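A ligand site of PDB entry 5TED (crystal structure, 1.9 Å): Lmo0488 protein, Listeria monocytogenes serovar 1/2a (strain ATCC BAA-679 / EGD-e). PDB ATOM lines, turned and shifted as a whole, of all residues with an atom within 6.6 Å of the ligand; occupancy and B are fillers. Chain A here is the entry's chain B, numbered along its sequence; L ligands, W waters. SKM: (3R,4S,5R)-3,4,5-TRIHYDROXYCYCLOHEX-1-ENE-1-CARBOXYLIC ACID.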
ATOM      1  N   ILE A  10     -32.626  13.305   1.452  1.00  0.00           N
ATOM      2  CA  ILE A  10     -31.527  13.003   0.544  1.00  0.00           C
ATOM      3  C   ILE A  10     -30.592  14.202   0.486  1.00  0.00           C
ATOM      4  O   ILE A  10     -31.008  15.361   0.615  1.00  0.00           O
ATOM      5  CB  ILE A  10     -32.050  12.622  -0.850  1.00  0.00           C
ATOM      6  CG1 ILE A  10     -32.917  13.748  -1.414  1.00  0.00           C
ATOM      7  CG2 ILE A  10     -32.852  11.347  -0.806  1.00  0.00           C
ATOM      8  CD1 ILE A  10     -33.488  13.445  -2.831  1.00  0.00           C
ATOM      9  N   TYR A  11     -29.300  13.916   0.277  1.00  0.00           N
ATOM     10  CA  TYR A  11     -28.235  14.876   0.486  1.00  0.00           C
ATOM     11  C   TYR A  11     -28.490  16.216  -0.200  1.00  0.00           C
ATOM     12  O   TYR A  11     -28.181  17.280   0.351  1.00  0.00           O
ATOM     13  CB  TYR A  11     -26.928  14.301  -0.023  1.00  0.00           C
ATOM     14  CG  TYR A  11     -26.464  13.068   0.692  1.00  0.00           C
ATOM     15  CD1 TYR A  11     -25.939  13.140   1.970  1.00  0.00           C
ATOM     16  CD2 TYR A  11     -26.530  11.825   0.065  1.00  0.00           C
ATOM     17  CE1 TYR A  11     -25.482  11.999   2.623  1.00  0.00           C
ATOM     18  CE2 TYR A  11     -26.075  10.667   0.714  1.00  0.00           C
ATOM     19  CZ  TYR A  11     -25.553  10.769   1.994  1.00  0.00           C
ATOM     20  OH  TYR A  11     -25.085   9.656   2.649  1.00  0.00           O
ATOM     21  N   THR A  12     -28.937  16.188  -1.454  1.00  0.00           N
ATOM     22  CA  THR A  12     -28.978  17.474  -2.141  1.00  0.00           C
ATOM     23  C   THR A  12     -29.969  18.434  -1.498  1.00  0.00           C
ATOM     24  O   THR A  12     -29.940  19.624  -1.824  1.00  0.00           O
ATOM     25  CB  THR A  12     -29.277  17.342  -3.646  1.00  0.00           C
ATOM     26  OG1 THR A  12     -30.554  16.732  -3.843  1.00  0.00           O
ATOM     27  CG2 THR A  12     -28.171  16.540  -4.375  1.00  0.00           C
ATOM     28  N   GLY A  41     -29.069  11.172   3.943  1.00  0.00           N
ATOM     29  CA  GLY A  41     -28.721   9.860   3.418  1.00  0.00           C
ATOM     30  C   GLY A  41     -29.310   9.629   2.036  1.00  0.00           C
ATOM     31  O   GLY A  41     -29.894  10.534   1.426  1.00  0.00           O
ATOM     32  N   ALA A  42     -29.136   8.400   1.544  1.00  0.00           N
ATOM     33  CA  ALA A  42     -29.706   7.969   0.271  1.00  0.00           C
ATOM     34  C   ALA A  42     -31.091   7.353   0.492  1.00  0.00           C
ATOM     35  O   ALA A  42     -31.427   6.878   1.583  1.00  0.00           O
ATOM     36  CB  ALA A  42     -28.791   6.956  -0.435  1.00  0.00           C
ATOM     37  N   THR A  43     -31.912   7.371  -0.573  1.00  0.00           N
ATOM     38  CA  THR A  43     -33.310   6.947  -0.484  1.00  0.00           C
ATOM     39  C   THR A  43     -33.457   5.540   0.086  1.00  0.00           C
ATOM     40  O   THR A  43     -34.366   5.267   0.882  1.00  0.00           O
ATOM     41  CB  THR A  43     -33.974   7.024  -1.860  1.00  0.00           C
ATOM     42  OG1 THR A  43     -34.094   8.382  -2.280  1.00  0.00           O
ATOM     43  CG2 THR A  43     -35.377   6.416  -1.825  1.00  0.00           C
ATOM     44  N   LYS A  44     -32.589   4.615  -0.334  1.00  0.00           N
ATOM     45  CA  LYS A  44     -32.801   3.236   0.069  1.00  0.00           C
ATOM     46  C   LYS A  44     -32.556   3.052   1.580  1.00  0.00           C
ATOM     47  O   LYS A  44     -33.232   2.232   2.209  1.00  0.00           O
ATOM     48  CB  LYS A  44     -31.919   2.313  -0.779  1.00  0.00           C
ATOM     49  CG  LYS A  44     -32.388   2.234  -2.253  1.00  0.00           C
ATOM     50  CD  LYS A  44     -33.856   1.764  -2.368  1.00  0.00           C
ATOM     51  CE  LYS A  44     -34.316   1.567  -3.823  1.00  0.00           C
ATOM     52  NZ  LYS A  44     -34.707   2.823  -4.553  1.00  0.00           N
ATOM     53  N   ILE A  46     -33.166   5.652   3.712  1.00  0.00           N
ATOM     54  CA  ILE A  46     -34.171   6.511   4.332  1.00  0.00           C
ATOM     55  C   ILE A  46     -35.487   5.769   4.539  1.00  0.00           C
ATOM     56  O   ILE A  46     -36.180   5.960   5.548  1.00  0.00           O
ATOM     57  CB  ILE A  46     -34.367   7.788   3.490  1.00  0.00           C
ATOM     58  CG1 ILE A  46     -33.192   8.751   3.725  1.00  0.00           C
ATOM     59  CG2 ILE A  46     -35.738   8.431   3.758  1.00  0.00           C
ATOM     60  CD1 ILE A  46     -33.125   9.921   2.740  1.00  0.00           C
ATOM     61  N   CYS A  60     -37.376  12.427  -0.238  1.00  0.00           N
ATOM     62  CA  CYS A  60     -36.557  11.449  -0.958  1.00  0.00           C
ATOM     63  C   CYS A  60     -37.184  11.127  -2.309  1.00  0.00           C
ATOM     64  O   CYS A  60     -38.170  11.750  -2.736  1.00  0.00           O
ATOM     65  CB  CYS A  60     -36.374  10.183  -0.105  1.00  0.00           C
ATOM     66  SG  CYS A  60     -37.905   9.284   0.167  1.00  0.00           S
ATOM     67  N   SER A  61     -36.583  10.157  -3.006  1.00  0.00           N
ATOM     68  CA  SER A  61     -37.074   9.689  -4.299  1.00  0.00           C
ATOM     69  C   SER A  61     -38.272   8.758  -4.098  1.00  0.00           C
ATOM     70  O   SER A  61     -38.401   8.090  -3.072  1.00  0.00           O
ATOM     71  CB  SER A  61     -35.988   8.929  -5.072  1.00  0.00           C
ATOM     72  OG  SER A  61     -34.879   9.783  -5.379  1.00  0.00           O
ATOM     73  N   GLN A  77     -35.790  18.263  -9.794  1.00  0.00           N
ATOM     74  CA  GLN A  77     -34.441  18.640 -10.206  1.00  0.00           C
ATOM     75  C   GLN A  77     -34.276  18.385 -11.695  1.00  0.00           C
ATOM     76  O   GLN A  77     -35.030  17.619 -12.308  1.00  0.00           O
ATOM     77  CB  GLN A  77     -33.371  17.866  -9.419  1.00  0.00           C
ATOM     78  CG  GLN A  77     -33.380  18.179  -7.944  1.00  0.00           C
ATOM     79  CD  GLN A  77     -32.451  17.306  -7.157  1.00  0.00           C
ATOM     80  OE1 GLN A  77     -32.302  16.105  -7.439  1.00  0.00           O
ATOM     81  NE2 GLN A  77     -31.801  17.895  -6.165  1.00  0.00           N
ATOM     82  N   PHE A 108     -23.879   6.662  -9.843  1.00  0.00           N
ATOM     83  CA  PHE A 108     -24.491   6.535  -8.524  1.00  0.00           C
ATOM     84  C   PHE A 108     -24.599   5.077  -8.126  1.00  0.00           C
ATOM     85  O   PHE A 108     -24.935   4.220  -8.944  1.00  0.00           O
ATOM     86  CB  PHE A 108     -25.879   7.175  -8.499  1.00  0.00           C
ATOM     87  CG  PHE A 108     -25.851   8.678  -8.377  1.00  0.00           C
ATOM     88  CD1 PHE A 108     -25.444   9.278  -7.197  1.00  0.00           C
ATOM     89  CD2 PHE A 108     -26.195   9.479  -9.455  1.00  0.00           C
ATOM     90  CE1 PHE A 108     -25.403  10.670  -7.092  1.00  0.00           C
ATOM     91  CE2 PHE A 108     -26.148  10.858  -9.349  1.00  0.00           C
ATOM     92  CZ  PHE A 108     -25.763  11.449  -8.166  1.00  0.00           C
ATOM     93  N   SER A 109     -24.313   4.784  -6.850  1.00  0.00           N
ATOM     94  CA  SER A 109     -24.450   3.431  -6.340  1.00  0.00           C
ATOM     95  C   SER A 109     -25.926   3.025  -6.281  1.00  0.00           C
ATOM     96  O   SER A 109     -26.829   3.854  -6.400  1.00  0.00           O
ATOM     97  CB  SER A 109     -23.840   3.316  -4.948  1.00  0.00           C
ATOM     98  OG  SER A 109     -24.479   4.222  -4.072  1.00  0.00           O
ATOM     99  N   THR A 111     -27.710   2.290  -3.838  1.00  0.00           N
ATOM    100  CA  THR A 111     -28.472   2.905  -2.755  1.00  0.00           C
ATOM    101  C   THR A 111     -29.197   4.179  -3.191  1.00  0.00           C
ATOM    102  O   THR A 111     -30.096   4.644  -2.475  1.00  0.00           O
ATOM    103  CB  THR A 111     -27.551   3.216  -1.573  1.00  0.00           C
ATOM    104  OG1 THR A 111     -26.493   4.076  -2.010  1.00  0.00           O
ATOM    105  CG2 THR A 111     -26.939   1.935  -1.004  1.00  0.00           C
ATOM    106  N   SER A 112     -28.840   4.742  -4.346  1.00  0.00           N
ATOM    107  CA  SER A 112     -29.369   6.033  -4.765  1.00  0.00           C
ATOM    108  C   SER A 112     -30.792   5.873  -5.311  1.00  0.00           C
ATOM    109  O   SER A 112     -31.010   5.117  -6.261  1.00  0.00           O
ATOM    110  CB  SER A 112     -28.485   6.652  -5.837  1.00  0.00           C
ATOM    111  OG  SER A 112     -29.028   7.890  -6.255  1.00  0.00           O
ATOM    112  N   GLY A 113     -31.735   6.632  -4.736  1.00  0.00           N
ATOM    113  CA  GLY A 113     -33.072   6.693  -5.285  1.00  0.00           C
ATOM    114  C   GLY A 113     -33.152   7.314  -6.662  1.00  0.00           C
ATOM    115  O   GLY A 113     -34.214   7.224  -7.298  1.00  0.00           O
ATOM    116  N   LEU A 114     -32.054   7.900  -7.159  1.00  0.00           N
ATOM    117  CA  LEU A 114     -32.022   8.392  -8.536  1.00  0.00           C
ATOM    118  C   LEU A 114     -31.796   7.289  -9.554  1.00  0.00           C
ATOM    119  O   LEU A 114     -32.043   7.505 -10.747  1.00  0.00           O
ATOM    120  CB  LEU A 114     -30.901   9.424  -8.690  1.00  0.00           C
ATOM    121  CG  LEU A 114     -31.260  10.880  -8.914  1.00  0.00           C
ATOM    122  CD1 LEU A 114     -29.986  11.640  -9.253  1.00  0.00           C
ATOM    123  CD2 LEU A 114     -32.289  11.022 -10.023  1.00  0.00           C
ATOM    124  N   ARG A 115     -31.331   6.110  -9.136  1.00  0.00           N
ATOM    125  CA  ARG A 115     -30.902   5.128 -10.126  1.00  0.00           C
ATOM    126  C   ARG A 115     -32.024   4.592 -11.003  1.00  0.00           C
ATOM    127  O   ARG A 115     -31.793   4.358 -12.197  1.00  0.00           O
ATOM    128  CB  ARG A 115     -30.169   3.961  -9.452  1.00  0.00           C
ATOM    129  CG  ARG A 115     -28.696   4.261  -9.166  1.00  0.00           C
ATOM    130  CD  ARG A 115     -27.846   4.271 -10.434  1.00  0.00           C
ATOM    131  NE  ARG A 115     -27.991   3.003 -11.139  1.00  0.00           N
ATOM    132  CZ  ARG A 115     -27.427   1.875 -10.718  1.00  0.00           C
ATOM    133  NH1 ARG A 115     -26.658   1.882  -9.628  1.00  0.00           N
ATOM    134  NH2 ARG A 115     -27.617   0.744 -11.394  1.00  0.00           N
ATOM    135  N   VAL A 135     -20.210   6.078  -6.623  1.00  0.00           N
ATOM    136  CA  VAL A 135     -20.242   6.937  -5.442  1.00  0.00           C
ATOM    137  C   VAL A 135     -21.704   7.128  -5.039  1.00  0.00           C
ATOM    138  O   VAL A 135     -22.621   6.993  -5.863  1.00  0.00           O
ATOM    139  CB  VAL A 135     -19.584   8.338  -5.640  1.00  0.00           C
ATOM    140  CG1 VAL A 135     -18.356   8.248  -6.531  1.00  0.00           C
ATOM    141  CG2 VAL A 135     -20.568   9.330  -6.197  1.00  0.00           C
ATOM    142  N   GLU A 136     -21.916   7.484  -3.785  1.00  0.00           N
ATOM    143  CA  GLU A 136     -23.265   7.724  -3.275  1.00  0.00           C
ATOM    144  C   GLU A 136     -23.616   9.206  -3.218  1.00  0.00           C
ATOM    145  O   GLU A 136     -24.683   9.605  -3.688  1.00  0.00           O
ATOM    146  CB  GLU A 136     -23.442   7.102  -1.888  1.00  0.00           C
ATOM    147  CG  GLU A 136     -24.831   7.390  -1.328  1.00  0.00           C
ATOM    148  CD  GLU A 136     -25.117   6.637  -0.034  1.00  0.00           C
ATOM    149  OE1 GLU A 136     -25.063   7.269   1.038  1.00  0.00           O
ATOM    150  OE2 GLU A 136     -25.365   5.405  -0.111  1.00  0.00           O
ATOM    151  N   GLU A 137     -22.731  10.029  -2.681  1.00  0.00           N
ATOM    152  CA  GLU A 137     -23.049  11.420  -2.394  1.00  0.00           C
ATOM    153  C   GLU A 137     -22.527  12.353  -3.489  1.00  0.00           C
ATOM    154  O   GLU A 137     -21.548  12.048  -4.171  1.00  0.00           O
ATOM    155  CB  GLU A 137     -22.488  11.777  -1.024  1.00  0.00           C
ATOM    156  CG  GLU A 137     -22.759  13.177  -0.591  1.00  0.00           C
ATOM    157  CD  GLU A 137     -21.615  14.090  -0.919  1.00  0.00           C
ATOM    158  OE1 GLU A 137     -20.543  13.565  -1.286  1.00  0.00           O
ATOM    159  OE2 GLU A 137     -21.794  15.319  -0.800  1.00  0.00           O
ATOM    160  N   ASP A 138     -23.200  13.493  -3.652  1.00  0.00           N
ATOM    161  CA  ASP A 138     -23.010  14.297  -4.868  1.00  0.00           C
ATOM    162  C   ASP A 138     -21.694  15.040  -4.864  1.00  0.00           C
ATOM    163  O   ASP A 138     -21.069  15.186  -5.924  1.00  0.00           O
ATOM    164  CB  ASP A 138     -24.178  15.264  -5.033  1.00  0.00           C
ATOM    165  CG  ASP A 138     -25.512  14.572  -4.878  1.00  0.00           C
ATOM    166  OD1 ASP A 138     -25.888  14.309  -3.720  1.00  0.00           O
ATOM    167  OD2 ASP A 138     -26.138  14.251  -5.914  1.00  0.00           O
ATOM    168  N   MET A 154     -26.032  13.757 -13.132  1.00  0.00           N
ATOM    169  CA  MET A 154     -26.376  14.066 -11.745  1.00  0.00           C
ATOM    170  C   MET A 154     -27.325  15.249 -11.732  1.00  0.00           C
ATOM    171  O   MET A 154     -27.495  15.921 -12.746  1.00  0.00           O
ATOM    172  CB  MET A 154     -25.126  14.346 -10.902  1.00  0.00           C
ATOM    173  CG  MET A 154     -24.337  15.561 -11.340  1.00  0.00           C
ATOM    174  SD  MET A 154     -22.695  15.701 -10.578  1.00  0.00           S
ATOM    175  CE  MET A 154     -23.135  15.743  -8.837  1.00  0.00           C
ATOM    176  N   PRO A 155     -27.937  15.555 -10.591  1.00  0.00           N
ATOM    177  CA  PRO A 155     -28.802  16.740 -10.509  1.00  0.00           C
ATOM    178  C   PRO A 155     -28.002  18.013 -10.675  1.00  0.00           C
ATOM    179  O   PRO A 155     -26.882  18.124 -10.175  1.00  0.00           O
ATOM    180  CB  PRO A 155     -29.416  16.658  -9.096  1.00  0.00           C
ATOM    181  CG  PRO A 155     -29.044  15.349  -8.545  1.00  0.00           C
ATOM    182  CD  PRO A 155     -27.822  14.858  -9.296  1.00  0.00           C
ATOM    183  N   ARG A 177     -37.316  14.595 -12.954  1.00  0.00           N
ATOM    184  CA  ARG A 177     -36.799  14.052 -11.698  1.00  0.00           C
ATOM    185  C   ARG A 177     -37.609  14.732 -10.607  1.00  0.00           C
ATOM    186  O   ARG A 177     -37.397  15.903 -10.316  1.00  0.00           O
ATOM    187  CB  ARG A 177     -35.302  14.337 -11.547  1.00  0.00           C
ATOM    188  CG  ARG A 177     -34.590  13.632 -10.382  1.00  0.00           C
ATOM    189  CD  ARG A 177     -35.107  14.097  -8.999  1.00  0.00           C
ATOM    190  NE  ARG A 177     -34.144  13.840  -7.918  1.00  0.00           N
ATOM    191  CZ  ARG A 177     -34.086  12.727  -7.189  1.00  0.00           C
ATOM    192  NH1 ARG A 177     -34.948  11.739  -7.400  1.00  0.00           N
ATOM    193  NH2 ARG A 177     -33.170  12.611  -6.225  1.00  0.00           N
ATOM    194  N   ILE A 179     -38.999  14.873  -6.548  1.00  0.00           N
ATOM    195  CA  ILE A 179     -38.637  14.558  -5.172  1.00  0.00           C
ATOM    196  C   ILE A 179     -39.890  14.690  -4.313  1.00  0.00           C
ATOM    197  O   ILE A 179     -40.684  15.624  -4.488  1.00  0.00           O
ATOM    198  CB  ILE A 179     -37.511  15.499  -4.668  1.00  0.00           C
ATOM    199  CG1 ILE A 179     -36.209  15.175  -5.392  1.00  0.00           C
ATOM    200  CG2 ILE A 179     -37.361  15.407  -3.136  1.00  0.00           C
ATOM    201  CD1 ILE A 179     -35.115  16.167  -5.131  1.00  0.00           C
HETATM  202  O12 SKM L   1     -27.772  12.665  -3.252  1.00  0.00           O
HETATM  203  C8  SKM L   1     -27.506  11.589  -4.148  1.00  0.00           C
HETATM  204  C6  SKM L   1     -27.633  10.372  -3.531  1.00  0.00           C
HETATM  205  O7  SKM L   1     -27.374   9.300  -4.438  1.00  0.00           O
HETATM  206  C5  SKM L   1     -29.150  10.084  -2.928  1.00  0.00           C
HETATM  207  C4  SKM L   1     -30.209  10.323  -3.917  1.00  0.00           C
HETATM  208  C1  SKM L   1     -31.619   9.747  -3.728  1.00  0.00           C
HETATM  209  O2  SKM L   1     -31.776   8.769  -2.955  1.00  0.00           O
HETATM  210  O3  SKM L   1     -32.595  10.233  -4.379  1.00  0.00           O
HETATM  211  C10 SKM L   1     -29.903  11.273  -5.171  1.00  0.00           C
HETATM  212  C9  SKM L   1     -28.567  11.709  -5.461  1.00  0.00           C
HETATM  213  O11 SKM L   1     -28.615  13.013  -5.875  1.00  0.00           O
HETATM  214  O   HOH W   1     -31.123  14.421  -5.875  1.00  0.00           O
HETATM  215  O   HOH W   2     -29.975  13.954  -3.077  1.00  0.00           O
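Residues that only touch the ligand: Phe 108 (3.4 Å), Ile 10 (3.5 Å), Pro 155 (3.6 Å), Tyr 11 (3.6 Å), Leu 114 (3.7 Å), Ala 42 (3.8 Å) and Thr 12 (3.9 Å). Within 4 Å of the ligand: Ile 10, Tyr 11, Thr 12, Ala 42, Thr 43, Ser 61, Phe 108, Ser 112, Gly 113, Leu 114, Glu 136, Asp 138, Pro 155 and Arg 177.
Water W2 lies within hydrogen-bond range of O12 of the ligand (2.6 Å), OG1 of Thr 12 (2.9 Å) and N of Tyr 11 (3.4 Å). Water W1 lies within hydrogen-bond range of the side-chain amide oxygen (OE1) of Gln 77 (2.6 Å), the guanidinium group (NH2) of Arg 177 (2.8 Å), an oxygen (O11) of the ligand (2.9 Å) and the side-chain hydroxyl (OG1) of Thr 12 (3.1 Å).
The backbone NH (N) of Thr 43 lies within hydrogen-bond range of an oxygen (O2) of the ligand (2.8 Å). An oxygen (O2) of the ligand sits at hydrogen-bond distance from the side-chain hydroxyl (OG1) of Thr 43, 2.4 Å away. OG of Ser 61 is in hydrogen-bond range of O3 of the ligand. An oxygen (O12) of the ligand sits at hydrogen-bond distance from the side-chain carboxylate (OD1) of Asp 138, at 2.5 Å. The backbone NH of Gly 113 sits at hydrogen-bond distance from an oxygen (O2) of the ligand (2.8 Å). O7 of the ligand sits at hydrogen-bond distance from O of Glu 136, 2.8 Å away. The side-chain hydroxyl (OG) of Ser 112 sits at hydrogen-bond distance from an oxygen (O7) of the ligand. O3 of the ligand lies within salt-bridge range of NH2 of Arg 177, 3.1 Å away.
OG1 of Thr 43 sits at hydrogen-bond distance from N of Ser 61. The side-chain hydroxyl of Ser 61 is in hydrogen-bond range of the backbone carbonyl oxygen of Gly 113 (3.3 Å). The side-chain hydroxyl of Ser 61 sits at hydrogen-bond distance from the guanidinium group of Arg 177, at 2.8 Å. The side-chain hydroxyl of Tyr 11 sits at hydrogen-bond distance from the side-chain carboxylate of Glu 136 (2.9 Å). OE2 of Glu 136 lies within hydrogen-bond range of OG1 of Thr 111, at 2.6 Å. O of Arg 177 lies within hydrogen-bond range of N of Gln 77, 2.9 Å away. The guanidinium group of Arg 115 sits at hydrogen-bond distance from the backbone carbonyl oxygen of Phe 108. OG1 of Thr 12 is in hydrogen-bond range of NE2 of Gln 77 (2.9 Å).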
